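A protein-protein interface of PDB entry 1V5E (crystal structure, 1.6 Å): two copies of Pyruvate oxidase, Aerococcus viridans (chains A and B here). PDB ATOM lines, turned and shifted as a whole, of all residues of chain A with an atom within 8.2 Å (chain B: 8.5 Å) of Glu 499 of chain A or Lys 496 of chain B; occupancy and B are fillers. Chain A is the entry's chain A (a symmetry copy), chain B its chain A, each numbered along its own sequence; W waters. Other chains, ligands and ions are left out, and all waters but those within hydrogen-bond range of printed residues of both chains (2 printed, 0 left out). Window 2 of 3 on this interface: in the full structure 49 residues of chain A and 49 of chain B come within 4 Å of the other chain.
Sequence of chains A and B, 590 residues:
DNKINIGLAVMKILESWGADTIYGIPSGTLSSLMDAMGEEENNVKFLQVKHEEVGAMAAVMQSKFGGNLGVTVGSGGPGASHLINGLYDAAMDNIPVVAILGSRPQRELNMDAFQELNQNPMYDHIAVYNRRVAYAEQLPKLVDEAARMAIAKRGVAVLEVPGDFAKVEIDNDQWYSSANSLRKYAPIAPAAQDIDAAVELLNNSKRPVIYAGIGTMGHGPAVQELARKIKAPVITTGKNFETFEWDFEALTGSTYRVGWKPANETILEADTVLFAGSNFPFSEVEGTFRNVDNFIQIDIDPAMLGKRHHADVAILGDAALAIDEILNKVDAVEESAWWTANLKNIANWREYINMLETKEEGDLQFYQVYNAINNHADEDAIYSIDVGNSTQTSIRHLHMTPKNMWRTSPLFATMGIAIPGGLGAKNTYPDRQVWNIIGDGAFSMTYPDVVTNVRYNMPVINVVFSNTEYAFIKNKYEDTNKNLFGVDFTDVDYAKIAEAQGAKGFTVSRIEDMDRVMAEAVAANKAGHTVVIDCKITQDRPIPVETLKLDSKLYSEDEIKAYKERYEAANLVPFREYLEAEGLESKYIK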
ATOM      1  N   VAL A 450      32.541  21.148  26.613  1.00  0.00           N
ATOM      2  CA  VAL A 450      33.322  21.547  25.451  1.00  0.00           C
ATOM      3  C   VAL A 450      33.767  22.975  25.749  1.00  0.00           C
ATOM      4  O   VAL A 450      34.860  23.394  25.364  1.00  0.00           O
ATOM      5  CB  VAL A 450      32.470  21.530  24.159  1.00  0.00           C
ATOM      6  CG1 VAL A 450      33.159  22.334  23.057  1.00  0.00           C
ATOM      7  CG2 VAL A 450      32.264  20.100  23.702  1.00  0.00           C
ATOM      8  N   VAL A 454      37.369  25.568  25.552  1.00  0.00           N
ATOM      9  CA  VAL A 454      37.337  26.915  25.001  1.00  0.00           C
ATOM     10  C   VAL A 454      37.859  27.930  26.014  1.00  0.00           C
ATOM     11  O   VAL A 454      38.770  28.707  25.719  1.00  0.00           O
ATOM     12  CB  VAL A 454      35.898  27.324  24.604  1.00  0.00           C
ATOM     13  CG1 VAL A 454      35.888  28.762  24.108  1.00  0.00           C
ATOM     14  CG2 VAL A 454      35.362  26.397  23.528  1.00  0.00           C
ATOM     15  N   ASP A 493      21.723  19.210  16.509  1.00  0.00           N
ATOM     16  CA  ASP A 493      22.760  19.880  15.729  1.00  0.00           C
ATOM     17  C   ASP A 493      23.961  20.189  16.619  1.00  0.00           C
ATOM     18  O   ASP A 493      24.047  21.271  17.202  1.00  0.00           O
ATOM     19  CB  ASP A 493      22.212  21.183  15.151  1.00  0.00           C
ATOM     20  CG  ASP A 493      23.138  21.799  14.124  1.00  0.00           C
ATOM     21  OD1 ASP A 493      24.365  21.596  14.231  1.00  0.00           O
ATOM     22  OD2 ASP A 493      22.638  22.498  13.218  1.00  0.00           O
ATOM     23  N   TYR A 494      24.890  19.245  16.722  1.00  0.00           N
ATOM     24  CA  TYR A 494      26.063  19.445  17.568  1.00  0.00           C
ATOM     25  C   TYR A 494      26.980  20.572  17.101  1.00  0.00           C
ATOM     26  O   TYR A 494      27.646  21.208  17.916  1.00  0.00           O
ATOM     27  CB  TYR A 494      26.852  18.140  17.690  1.00  0.00           C
ATOM     28  CG  TYR A 494      26.043  17.026  18.309  1.00  0.00           C
ATOM     29  CD1 TYR A 494      25.795  15.849  17.607  1.00  0.00           C
ATOM     30  CD2 TYR A 494      25.485  17.166  19.583  1.00  0.00           C
ATOM     31  CE1 TYR A 494      25.008  14.838  18.152  1.00  0.00           C
ATOM     32  CE2 TYR A 494      24.695  16.159  20.138  1.00  0.00           C
ATOM     33  CZ  TYR A 494      24.461  15.002  19.416  1.00  0.00           C
ATOM     34  OH  TYR A 494      23.668  14.010  19.944  1.00  0.00           O
ATOM     35  N   ALA A 495      27.014  20.823  15.797  1.00  0.00           N
ATOM     36  CA  ALA A 495      27.853  21.892  15.264  1.00  0.00           C
ATOM     37  C   ALA A 495      27.343  23.237  15.770  1.00  0.00           C
ATOM     38  O   ALA A 495      28.124  24.113  16.143  1.00  0.00           O
ATOM     39  CB  ALA A 495      27.841  21.865  13.735  1.00  0.00           C
ATOM     40  N   LYS A 496      26.022  23.392  15.788  1.00  0.00           N
ATOM     41  CA  LYS A 496      25.395  24.625  16.254  1.00  0.00           C
ATOM     42  C   LYS A 496      25.647  24.824  17.746  1.00  0.00           C
ATOM     43  O   LYS A 496      25.880  25.941  18.211  1.00  0.00           O
ATOM     44  CB  LYS A 496      23.892  24.580  15.971  1.00  0.00           C
ATOM     45  CG  LYS A 496      23.135  25.829  16.401  1.00  0.00           C
ATOM     46  CD  LYS A 496      21.714  25.812  15.863  1.00  0.00           C
ATOM     47  CE  LYS A 496      20.951  27.060  16.267  1.00  0.00           C
ATOM     48  NZ  LYS A 496      19.607  27.104  15.627  1.00  0.00           N
ATOM     49  N   ILE A 497      25.592  23.732  18.495  1.00  0.00           N
ATOM     50  CA  ILE A 497      25.840  23.792  19.926  1.00  0.00           C
ATOM     51  C   ILE A 497      27.278  24.238  20.157  1.00  0.00           C
ATOM     52  O   ILE A 497      27.549  25.086  21.009  1.00  0.00           O
ATOM     53  CB  ILE A 497      25.604  22.416  20.568  1.00  0.00           C
ATOM     54  CG1 ILE A 497      24.111  22.087  20.502  1.00  0.00           C
ATOM     55  CG2 ILE A 497      26.123  22.400  22.004  1.00  0.00           C
ATOM     56  CD1 ILE A 497      23.753  20.729  21.049  1.00  0.00           C
ATOM     57  N   ALA A 498      28.198  23.670  19.385  1.00  0.00           N
ATOM     58  CA  ALA A 498      29.606  24.015  19.507  1.00  0.00           C
ATOM     59  C   ALA A 498      29.800  25.516  19.294  1.00  0.00           C
ATOM     60  O   ALA A 498      30.500  26.173  20.062  1.00  0.00           O
ATOM     61  CB  ALA A 498      30.425  23.222  18.492  1.00  0.00           C
ATOM     62  N   GLU A 499      29.175  26.056  18.252  1.00  0.00           N
ATOM     63  CA  GLU A 499      29.282  27.484  17.965  1.00  0.00           C
ATOM     64  C   GLU A 499      28.764  28.303  19.139  1.00  0.00           C
ATOM     65  O   GLU A 499      29.331  29.339  19.488  1.00  0.00           O
ATOM     66  CB  GLU A 499      28.485  27.835  16.705  1.00  0.00           C
ATOM     67  CG  GLU A 499      29.069  27.259  15.427  1.00  0.00           C
ATOM     68  CD  GLU A 499      30.345  27.959  14.999  1.00  0.00           C
ATOM     69  OE1 GLU A 499      31.131  27.349  14.243  1.00  0.00           O
ATOM     70  OE2 GLU A 499      30.557  29.124  15.407  1.00  0.00           O
ATOM     71  N   ALA A 500      27.678  27.831  19.747  1.00  0.00           N
ATOM     72  CA  ALA A 500      27.080  28.518  20.885  1.00  0.00           C
ATOM     73  C   ALA A 500      28.002  28.504  22.100  1.00  0.00           C
ATOM     74  O   ALA A 500      27.865  29.334  23.001  1.00  0.00           O
ATOM     75  CB  ALA A 500      25.742  27.871  21.240  1.00  0.00           C
ATOM     76  N   GLN A 501      28.947  27.566  22.120  1.00  0.00           N
ATOM     77  CA  GLN A 501      29.888  27.438  23.233  1.00  0.00           C
ATOM     78  C   GLN A 501      31.221  28.128  22.975  1.00  0.00           C
ATOM     79  O   GLN A 501      32.118  28.092  23.821  1.00  0.00           O
ATOM     80  CB  GLN A 501      30.155  25.960  23.530  1.00  0.00           C
ATOM     81  CG  GLN A 501      28.918  25.149  23.856  1.00  0.00           C
ATOM     82  CD  GLN A 501      29.197  23.663  23.824  1.00  0.00           C
ATOM     83  OE1 GLN A 501      29.777  23.153  22.864  1.00  0.00           O
ATOM     84  NE2 GLN A 501      28.779  22.956  24.866  1.00  0.00           N
ATOM     85  N   GLY A 502      31.361  28.741  21.804  1.00  0.00           N
ATOM     86  CA  GLY A 502      32.604  29.417  21.479  1.00  0.00           C
ATOM     87  C   GLY A 502      33.570  28.526  20.721  1.00  0.00           C
ATOM     88  O   GLY A 502      34.723  28.896  20.488  1.00  0.00           O
ATOM     89  N   ALA A 503      33.107  27.340  20.341  1.00  0.00           N
ATOM     90  CA  ALA A 503      33.941  26.413  19.593  1.00  0.00           C
ATOM     91  C   ALA A 503      33.567  26.523  18.123  1.00  0.00           C
ATOM     92  O   ALA A 503      32.621  27.233  17.771  1.00  0.00           O
ATOM     93  CB  ALA A 503      33.722  24.986  20.093  1.00  0.00           C
ATOM     94  N   LYS A 504      34.315  25.834  17.267  1.00  0.00           N
ATOM     95  CA  LYS A 504      34.046  25.852  15.836  1.00  0.00           C
ATOM     96  C   LYS A 504      33.372  24.549  15.440  1.00  0.00           C
ATOM     97  O   LYS A 504      33.920  23.467  15.651  1.00  0.00           O
ATOM     98  CB  LYS A 504      35.349  26.025  15.054  1.00  0.00           C
ATOM     99  CG  LYS A 504      35.205  25.858  13.551  1.00  0.00           C
ATOM    100  CD  LYS A 504      34.287  26.898  12.931  1.00  0.00           C
ATOM    101  CE  LYS A 504      34.145  26.653  11.435  1.00  0.00           C
ATOM    102  NZ  LYS A 504      33.381  27.727  10.744  1.00  0.00           N
ATOM    103  N   GLY A 505      32.181  24.656  14.865  1.00  0.00           N
ATOM    104  CA  GLY A 505      31.462  23.461  14.469  1.00  0.00           C
ATOM    105  C   GLY A 505      31.422  23.174  12.981  1.00  0.00           C
ATOM    106  O   GLY A 505      31.349  24.089  12.154  1.00  0.00           O
ATOM    107  N   PHE A 506      31.482  21.888  12.650  1.00  0.00           N
ATOM    108  CA  PHE A 506      31.418  21.422  11.271  1.00  0.00           C
ATOM    109  C   PHE A 506      30.397  20.297  11.215  1.00  0.00           C
ATOM    110  O   PHE A 506      30.203  19.572  12.193  1.00  0.00           O
ATOM    111  CB  PHE A 506      32.766  20.863  10.797  1.00  0.00           C
ATOM    112  CG  PHE A 506      33.880  21.865  10.787  1.00  0.00           C
ATOM    113  CD1 PHE A 506      34.579  22.158  11.951  1.00  0.00           C
ATOM    114  CD2 PHE A 506      34.239  22.511   9.607  1.00  0.00           C
ATOM    115  CE1 PHE A 506      35.620  23.079  11.945  1.00  0.00           C
ATOM    116  CE2 PHE A 506      35.278  23.436   9.589  1.00  0.00           C
ATOM    117  CZ  PHE A 506      35.971  23.721  10.758  1.00  0.00           C
ATOM    118  N   HIS A 529      41.518  27.032  17.937  1.00  0.00           N
ATOM    119  CA  HIS A 529      40.110  26.773  18.223  1.00  0.00           C
ATOM    120  C   HIS A 529      39.801  25.323  18.581  1.00  0.00           C
ATOM    121  O   HIS A 529      40.405  24.395  18.045  1.00  0.00           O
ATOM    122  CB  HIS A 529      39.229  27.144  17.022  1.00  0.00           C
ATOM    123  CG  HIS A 529      39.208  28.606  16.705  1.00  0.00           C
ATOM    124  ND1 HIS A 529      40.283  29.265  16.151  1.00  0.00           N
ATOM    125  CD2 HIS A 529      38.236  29.536  16.860  1.00  0.00           C
ATOM    126  CE1 HIS A 529      39.975  30.537  15.974  1.00  0.00           C
ATOM    127  NE2 HIS A 529      38.739  30.729  16.396  1.00  0.00           N
ATOM    128  N   THR A 530      38.864  25.136  19.506  1.00  0.00           N
ATOM    129  CA  THR A 530      38.423  23.792  19.842  1.00  0.00           C
ATOM    130  C   THR A 530      37.389  23.538  18.754  1.00  0.00           C
ATOM    131  O   THR A 530      36.614  24.434  18.406  1.00  0.00           O
ATOM    132  CB  THR A 530      37.755  23.730  21.229  1.00  0.00           C
ATOM    133  OG1 THR A 530      38.770  23.754  22.239  1.00  0.00           O
ATOM    134  CG2 THR A 530      36.928  22.450  21.374  1.00  0.00           C
ATOM    135  N   VAL A 531      37.382  22.339  18.190  1.00  0.00           N
ATOM    136  CA  VAL A 531      36.439  22.057  17.124  1.00  0.00           C
ATOM    137  C   VAL A 531      35.557  20.859  17.416  1.00  0.00           C
ATOM    138  O   VAL A 531      35.916  19.979  18.197  1.00  0.00           O
ATOM    139  CB  VAL A 531      37.171  21.806  15.787  1.00  0.00           C
ATOM    140  CG1 VAL A 531      38.074  22.983  15.461  1.00  0.00           C
ATOM    141  CG2 VAL A 531      37.978  20.524  15.866  1.00  0.00           C
ATOM    142  N   VAL A 532      34.387  20.850  16.795  1.00  0.00           N
ATOM    143  CA  VAL A 532      33.454  19.747  16.941  1.00  0.00           C
ATOM    144  C   VAL A 532      33.005  19.387  15.536  1.00  0.00           C
ATOM    145  O   VAL A 532      32.385  20.203  14.844  1.00  0.00           O
ATOM    146  CB  VAL A 532      32.224  20.132  17.790  1.00  0.00           C
ATOM    147  CG1 VAL A 532      31.183  19.020  17.735  1.00  0.00           C
ATOM    148  CG2 VAL A 532      32.646  20.376  19.235  1.00  0.00           C
ATOM    149  N   ASP B 491      30.334  33.226  27.984  1.00  0.00           N
ATOM    150  CA  ASP B 491      28.951  33.573  27.670  1.00  0.00           C
ATOM    151  C   ASP B 491      28.341  32.595  26.669  1.00  0.00           C
ATOM    152  O   ASP B 491      28.259  32.880  25.475  1.00  0.00           O
ATOM    153  CB  ASP B 491      28.882  34.993  27.103  1.00  0.00           C
ATOM    154  CG  ASP B 491      27.484  35.378  26.667  1.00  0.00           C
ATOM    155  OD1 ASP B 491      26.569  35.367  27.518  1.00  0.00           O
ATOM    156  OD2 ASP B 491      27.297  35.691  25.471  1.00  0.00           O
ATOM    157  N   VAL B 492      27.911  31.440  27.165  1.00  0.00           N
ATOM    158  CA  VAL B 492      27.313  30.422  26.314  1.00  0.00           C
ATOM    159  C   VAL B 492      25.903  30.822  25.887  1.00  0.00           C
ATOM    160  O   VAL B 492      25.085  31.230  26.714  1.00  0.00           O
ATOM    161  CB  VAL B 492      27.263  29.063  27.042  1.00  0.00           C
ATOM    162  CG1 VAL B 492      26.588  28.023  26.167  1.00  0.00           C
ATOM    163  CG2 VAL B 492      28.675  28.622  27.397  1.00  0.00           C
ATOM    164  N   ASP B 493      25.628  30.702  24.591  1.00  0.00           N
ATOM    165  CA  ASP B 493      24.323  31.058  24.042  1.00  0.00           C
ATOM    166  C   ASP B 493      23.343  29.906  24.244  1.00  0.00           C
ATOM    167  O   ASP B 493      23.198  29.046  23.374  1.00  0.00           O
ATOM    168  CB  ASP B 493      24.453  31.354  22.549  1.00  0.00           C
ATOM    169  CG  ASP B 493      23.202  31.979  21.968  1.00  0.00           C
ATOM    170  OD1 ASP B 493      22.101  31.699  22.486  1.00  0.00           O
ATOM    171  OD2 ASP B 493      23.321  32.739  20.984  1.00  0.00           O
ATOM    172  N   TYR B 494      22.665  29.888  25.387  1.00  0.00           N
ATOM    173  CA  TYR B 494      21.720  28.813  25.675  1.00  0.00           C
ATOM    174  C   TYR B 494      20.520  28.772  24.735  1.00  0.00           C
ATOM    175  O   TYR B 494      19.967  27.704  24.480  1.00  0.00           O
ATOM    176  CB  TYR B 494      21.250  28.902  27.128  1.00  0.00           C
ATOM    177  CG  TYR B 494      22.383  28.775  28.117  1.00  0.00           C
ATOM    178  CD1 TYR B 494      22.670  29.805  29.010  1.00  0.00           C
ATOM    179  CD2 TYR B 494      23.201  27.642  28.130  1.00  0.00           C
ATOM    180  CE1 TYR B 494      23.745  29.715  29.890  1.00  0.00           C
ATOM    181  CE2 TYR B 494      24.280  27.542  29.008  1.00  0.00           C
ATOM    182  CZ  TYR B 494      24.545  28.583  29.882  1.00  0.00           C
ATOM    183  OH  TYR B 494      25.617  28.505  30.739  1.00  0.00           O
ATOM    184  N   ALA B 495      20.118  29.928  24.216  1.00  0.00           N
ATOM    185  CA  ALA B 495      18.986  29.981  23.297  1.00  0.00           C
ATOM    186  C   ALA B 495      19.339  29.234  22.015  1.00  0.00           C
ATOM    187  O   ALA B 495      18.522  28.496  21.464  1.00  0.00           O
ATOM    188  CB  ALA B 495      18.625  31.432  22.980  1.00  0.00           C
ATOM    189  N   LYS B 496      20.569  29.426  21.547  1.00  0.00           N
ATOM    190  CA  LYS B 496      21.045  28.771  20.332  1.00  0.00           C
ATOM    191  C   LYS B 496      21.135  27.262  20.538  1.00  0.00           C
ATOM    192  O   LYS B 496      20.817  26.475  19.646  1.00  0.00           O
ATOM    193  CB  LYS B 496      22.412  29.336  19.941  1.00  0.00           C
ATOM    194  CG  LYS B 496      23.000  28.736  18.672  1.00  0.00           C
ATOM    195  CD  LYS B 496      24.221  29.519  18.217  1.00  0.00           C
ATOM    196  CE  LYS B 496      24.808  28.943  16.942  1.00  0.00           C
ATOM    197  NZ  LYS B 496      25.918  29.791  16.427  1.00  0.00           N
ATOM    198  N   ILE B 497      21.581  26.863  21.721  1.00  0.00           N
ATOM    199  CA  ILE B 497      21.687  25.449  22.043  1.00  0.00           C
ATOM    200  C   ILE B 497      20.292  24.836  22.029  1.00  0.00           C
ATOM    201  O   ILE B 497      20.084  23.750  21.485  1.00  0.00           O
ATOM    202  CB  ILE B 497      22.331  25.263  23.426  1.00  0.00           C
ATOM    203  CG1 ILE B 497      23.796  25.698  23.353  1.00  0.00           C
ATOM    204  CG2 ILE B 497      22.195  23.814  23.888  1.00  0.00           C
ATOM    205  CD1 ILE B 497      24.530  25.620  24.667  1.00  0.00           C
ATOM    206  N   ALA B 498      19.335  25.543  22.620  1.00  0.00           N
ATOM    207  CA  ALA B 498      17.962  25.066  22.669  1.00  0.00           C
ATOM    208  C   ALA B 498      17.440  24.822  21.253  1.00  0.00           C
ATOM    209  O   ALA B 498      16.839  23.786  20.977  1.00  0.00           O
ATOM    210  CB  ALA B 498      17.085  26.084  23.394  1.00  0.00           C
ATOM    211  N   GLU B 499      17.674  25.778  20.359  1.00  0.00           N
ATOM    212  CA  GLU B 499      17.230  25.640  18.974  1.00  0.00           C
ATOM    213  C   GLU B 499      17.856  24.408  18.335  1.00  0.00           C
ATOM    214  O   GLU B 499      17.205  23.689  17.575  1.00  0.00           O
ATOM    215  CB  GLU B 499      17.609  26.885  18.166  1.00  0.00           C
ATOM    216  CG  GLU B 499      16.849  28.136  18.570  1.00  0.00           C
ATOM    217  CD  GLU B 499      15.397  28.106  18.129  1.00  0.00           C
ATOM    218  OE1 GLU B 499      14.580  28.836  18.730  1.00  0.00           O
ATOM    219  OE2 GLU B 499      15.075  27.364  17.174  1.00  0.00           O
ATOM    220  N   ALA B 500      19.127  24.170  18.647  1.00  0.00           N
ATOM    221  CA  ALA B 500      19.846  23.024  18.104  1.00  0.00           C
ATOM    222  C   ALA B 500      19.271  21.705  18.615  1.00  0.00           C
ATOM    223  O   ALA B 500      19.466  20.657  17.998  1.00  0.00           O
ATOM    224  CB  ALA B 500      21.327  23.119  18.464  1.00  0.00           C
ATOM    225  N   GLN B 501      18.557  21.762  19.737  1.00  0.00           N
ATOM    226  CA  GLN B 501      17.962  20.568  20.337  1.00  0.00           C
ATOM    227  C   GLN B 501      16.500  20.369  19.958  1.00  0.00           C
ATOM    228  O   GLN B 501      15.864  19.411  20.401  1.00  0.00           O
ATOM    229  CB  GLN B 501      18.063  20.638  21.863  1.00  0.00           C
ATOM    230  CG  GLN B 501      19.472  20.787  22.395  1.00  0.00           C
ATOM    231  CD  GLN B 501      19.483  21.168  23.859  1.00  0.00           C
ATOM    232  OE1 GLN B 501      18.792  22.102  24.270  1.00  0.00           O
ATOM    233  NE2 GLN B 501      20.272  20.457  24.654  1.00  0.00           N
ATOM    234  N   GLY B 502      15.961  21.281  19.154  1.00  0.00           N
ATOM    235  CA  GLY B 502      14.571  21.167  18.750  1.00  0.00           C
ATOM    236  C   GLY B 502      13.636  21.941  19.661  1.00  0.00           C
ATOM    237  O   GLY B 502      12.413  21.840  19.544  1.00  0.00           O
ATOM    238  N   ALA B 503      14.208  22.710  20.581  1.00  0.00           N
ATOM    239  CA  ALA B 503      13.408  23.508  21.496  1.00  0.00           C
ATOM    240  C   ALA B 503      13.380  24.937  20.973  1.00  0.00           C
ATOM    241  O   ALA B 503      14.056  25.255  19.991  1.00  0.00           O
ATOM    242  CB  ALA B 503      14.011  23.466  22.898  1.00  0.00           C
ATOM    243  N   LYS B 504      12.589  25.788  21.617  1.00  0.00           N
ATOM    244  CA  LYS B 504      12.488  27.185  21.216  1.00  0.00           C
ATOM    245  C   LYS B 504      13.279  28.041  22.191  1.00  0.00           C
ATOM    246  O   LYS B 504      13.016  28.031  23.394  1.00  0.00           O
ATOM    247  CB  LYS B 504      11.024  27.627  21.201  1.00  0.00           C
ATOM    248  CG  LYS B 504      10.822  29.117  20.988  1.00  0.00           C
ATOM    249  CD  LYS B 504      11.344  29.595  19.644  1.00  0.00           C
ATOM    250  CE  LYS B 504      11.156  31.100  19.507  1.00  0.00           C
ATOM    251  NZ  LYS B 504      11.507  31.606  18.152  1.00  0.00           N
ATOM    252  N   GLY B 505      14.248  28.781  21.668  1.00  0.00           N
ATOM    253  CA  GLY B 505      15.061  29.616  22.530  1.00  0.00           C
ATOM    254  C   GLY B 505      14.787  31.105  22.460  1.00  0.00           C
ATOM    255  O   GLY B 505      14.479  31.651  21.396  1.00  0.00           O
ATOM    256  N   PHE B 506      14.894  31.756  23.615  1.00  0.00           N
ATOM    257  CA  PHE B 506      14.702  33.195  23.733  1.00  0.00           C
ATOM    258  C   PHE B 506      15.873  33.749  24.530  1.00  0.00           C
ATOM    259  O   PHE B 506      16.437  33.060  25.383  1.00  0.00           O
ATOM    260  CB  PHE B 506      13.411  33.539  24.487  1.00  0.00           C
ATOM    261  CG  PHE B 506      12.159  33.063  23.815  1.00  0.00           C
ATOM    262  CD1 PHE B 506      11.727  31.753  23.969  1.00  0.00           C
ATOM    263  CD2 PHE B 506      11.405  33.933  23.032  1.00  0.00           C
ATOM    264  CE1 PHE B 506      10.561  31.309  23.356  1.00  0.00           C
ATOM    265  CE2 PHE B 506      10.236  33.500  22.412  1.00  0.00           C
ATOM    266  CZ  PHE B 506       9.812  32.188  22.573  1.00  0.00           C
ATOM    267  N   THR B 507      16.238  34.993  24.247  1.00  0.00           N
ATOM    268  CA  THR B 507      17.323  35.655  24.956  1.00  0.00           C
ATOM    269  C   THR B 507      16.789  37.016  25.383  1.00  0.00           C
ATOM    270  O   THR B 507      16.172  37.719  24.588  1.00  0.00           O
ATOM    271  CB  THR B 507      18.554  35.856  24.051  1.00  0.00           C
ATOM    272  OG1 THR B 507      18.955  34.594  23.499  1.00  0.00           O
ATOM    273  CG2 THR B 507      19.709  36.437  24.847  1.00  0.00           C
ATOM    274  N   VAL B 532      13.353  27.575  26.231  1.00  0.00           N
ATOM    275  CA  VAL B 532      14.486  27.915  27.074  1.00  0.00           C
ATOM    276  C   VAL B 532      14.634  29.424  26.991  1.00  0.00           C
ATOM    277  O   VAL B 532      14.898  29.972  25.914  1.00  0.00           O
ATOM    278  CB  VAL B 532      15.791  27.244  26.596  1.00  0.00           C
ATOM    279  CG1 VAL B 532      16.978  27.796  27.376  1.00  0.00           C
ATOM    280  CG2 VAL B 532      15.699  25.734  26.791  1.00  0.00           C
ATOM    281  N   ASP B 534      16.841  32.311  28.017  1.00  0.00           N
ATOM    282  CA  ASP B 534      18.168  32.643  28.517  1.00  0.00           C
ATOM    283  C   ASP B 534      18.082  34.066  29.048  1.00  0.00           C
ATOM    284  O   ASP B 534      18.072  35.028  28.280  1.00  0.00           O
ATOM    285  CB  ASP B 534      19.192  32.552  27.384  1.00  0.00           C
ATOM    286  CG  ASP B 534      20.625  32.688  27.871  1.00  0.00           C
ATOM    287  OD1 ASP B 534      20.840  32.881  29.085  1.00  0.00           O
ATOM    288  OD2 ASP B 534      21.544  32.599  27.028  1.00  0.00           O
ATOM    289  N   LYS B 536      19.791  36.950  30.611  1.00  0.00           N
ATOM    290  CA  LYS B 536      21.105  37.518  30.881  1.00  0.00           C
ATOM    291  C   LYS B 536      20.915  38.581  31.954  1.00  0.00           C
ATOM    292  O   LYS B 536      20.606  39.735  31.648  1.00  0.00           O
ATOM    293  CB  LYS B 536      21.677  38.152  29.610  1.00  0.00           C
ATOM    294  CG  LYS B 536      21.740  37.221  28.404  1.00  0.00           C
ATOM    295  CD  LYS B 536      22.698  36.062  28.631  1.00  0.00           C
ATOM    296  CE  LYS B 536      22.864  35.227  27.370  1.00  0.00           C
ATOM    297  NZ  LYS B 536      23.860  34.133  27.556  1.00  0.00           N
HETATM  298  O   HOH W   1      27.143  31.247  18.288  1.00  0.00           O
HETATM  299  O   HOH W   2      18.625  24.720  14.968  1.00  0.00           O
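Among the printed residues, pairs that only touch across the chains: Lys 496 of chain A with Glu 499 of chain B (3.2 Å), Glu 499 of chain A with Lys 496 of chain B (3.2 Å), Lys 496 of chain A with Lys 496 of chain B (3.4 Å), Ala 500 of chain A with Val 492 of chain B (3.5 Å), Ile 497 of chain A with Ala 500 of chain B (3.6 Å), Ala 500 of chain A with Ile 497 of chain B (3.6 Å), Lys 496 of chain A with Ala 500 of chain B (3.8 Å) and Ala 500 of chain A with Lys 496 of chain B (3.8 Å).
The backbone NH (N) of Asp 493 of chain A sits at hydrogen-bond distance from the backbone carbonyl oxygen (O) of Ala 500 of chain B (3.1 Å). N of Asp 493 of chain B is in hydrogen-bond range of O of Ala 500 of chain A (3.1 Å).
Of chain B, only Lys 496 comes within 4 Å of Glu 499 of chain A. Lys 496 of chain B touches just these residues of chain A: Lys 496, Glu 499 and Ala 500. Of the printed residues of chain B, Ala 500 of chain A touches Val 492, Asp 493, Lys 496 and Ile 497. No residue of chain A comes within 4 Å of Ala 495 of chain B. Printed residues of chain A within 4 Å of Val 492 of chain B: Ala 500 (3.5 Å). Of the printed residues of chain A, Asp 493 of chain B touches Ala 500 (3.1 Å). Of the printed residues of chain B, Lys 496 of chain A touches Lys 496 (3.4 Å), Glu 499 (3.2 Å) and Ala 500 (3.8 Å). The nearest printed residue of chain A that does not touch Ile 497 of chain B is Ile 497 of chain A (4.3 Å).
Of the 20 printed residues of chain B, 6 touch a printed residue of chain A. Hydrophobic or aromatic side chains of chain B that line the printed part of chain A: Val 492, Ile 497 and Ala 500. Among the printed residues, no Asp or Glu carboxylate lies within 4 Å of a Lys or Arg side-chain nitrogen of the other chain.
Ile 497 of chain A touches Ala 500 of chain B, and with the chains exchanged Ala 500 of chain A touches Ile 497 of chain B. Of the 10 pairs that touch across the chains among the printed residues, 9 have their exchanged pair printed and touching as well.
The backbone carbonyl oxygen (O) of Ile 497 of chain A sits close to the side-chain amide oxygen (OE1) of Gln 501 of chain A, 3.5 Å away. O of Ile 497 of chain B lies close to OE1 of Gln 501 of chain B (3.5 Å). The backbone NH (N) of Lys 496 of chain B sits at hydrogen-bond distance from the side-chain carboxylate (OD1) of Asp 493 of chain B (2.9 Å).
Water W1 lies within hydrogen-bond range of the side-chain amino group of Lys 496 of chain B and the backbone carbonyl oxygen of Glu 499 of chain A. Water W2 bridges NZ of Lys 496 of chain A and O of Glu 499 of chain B.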
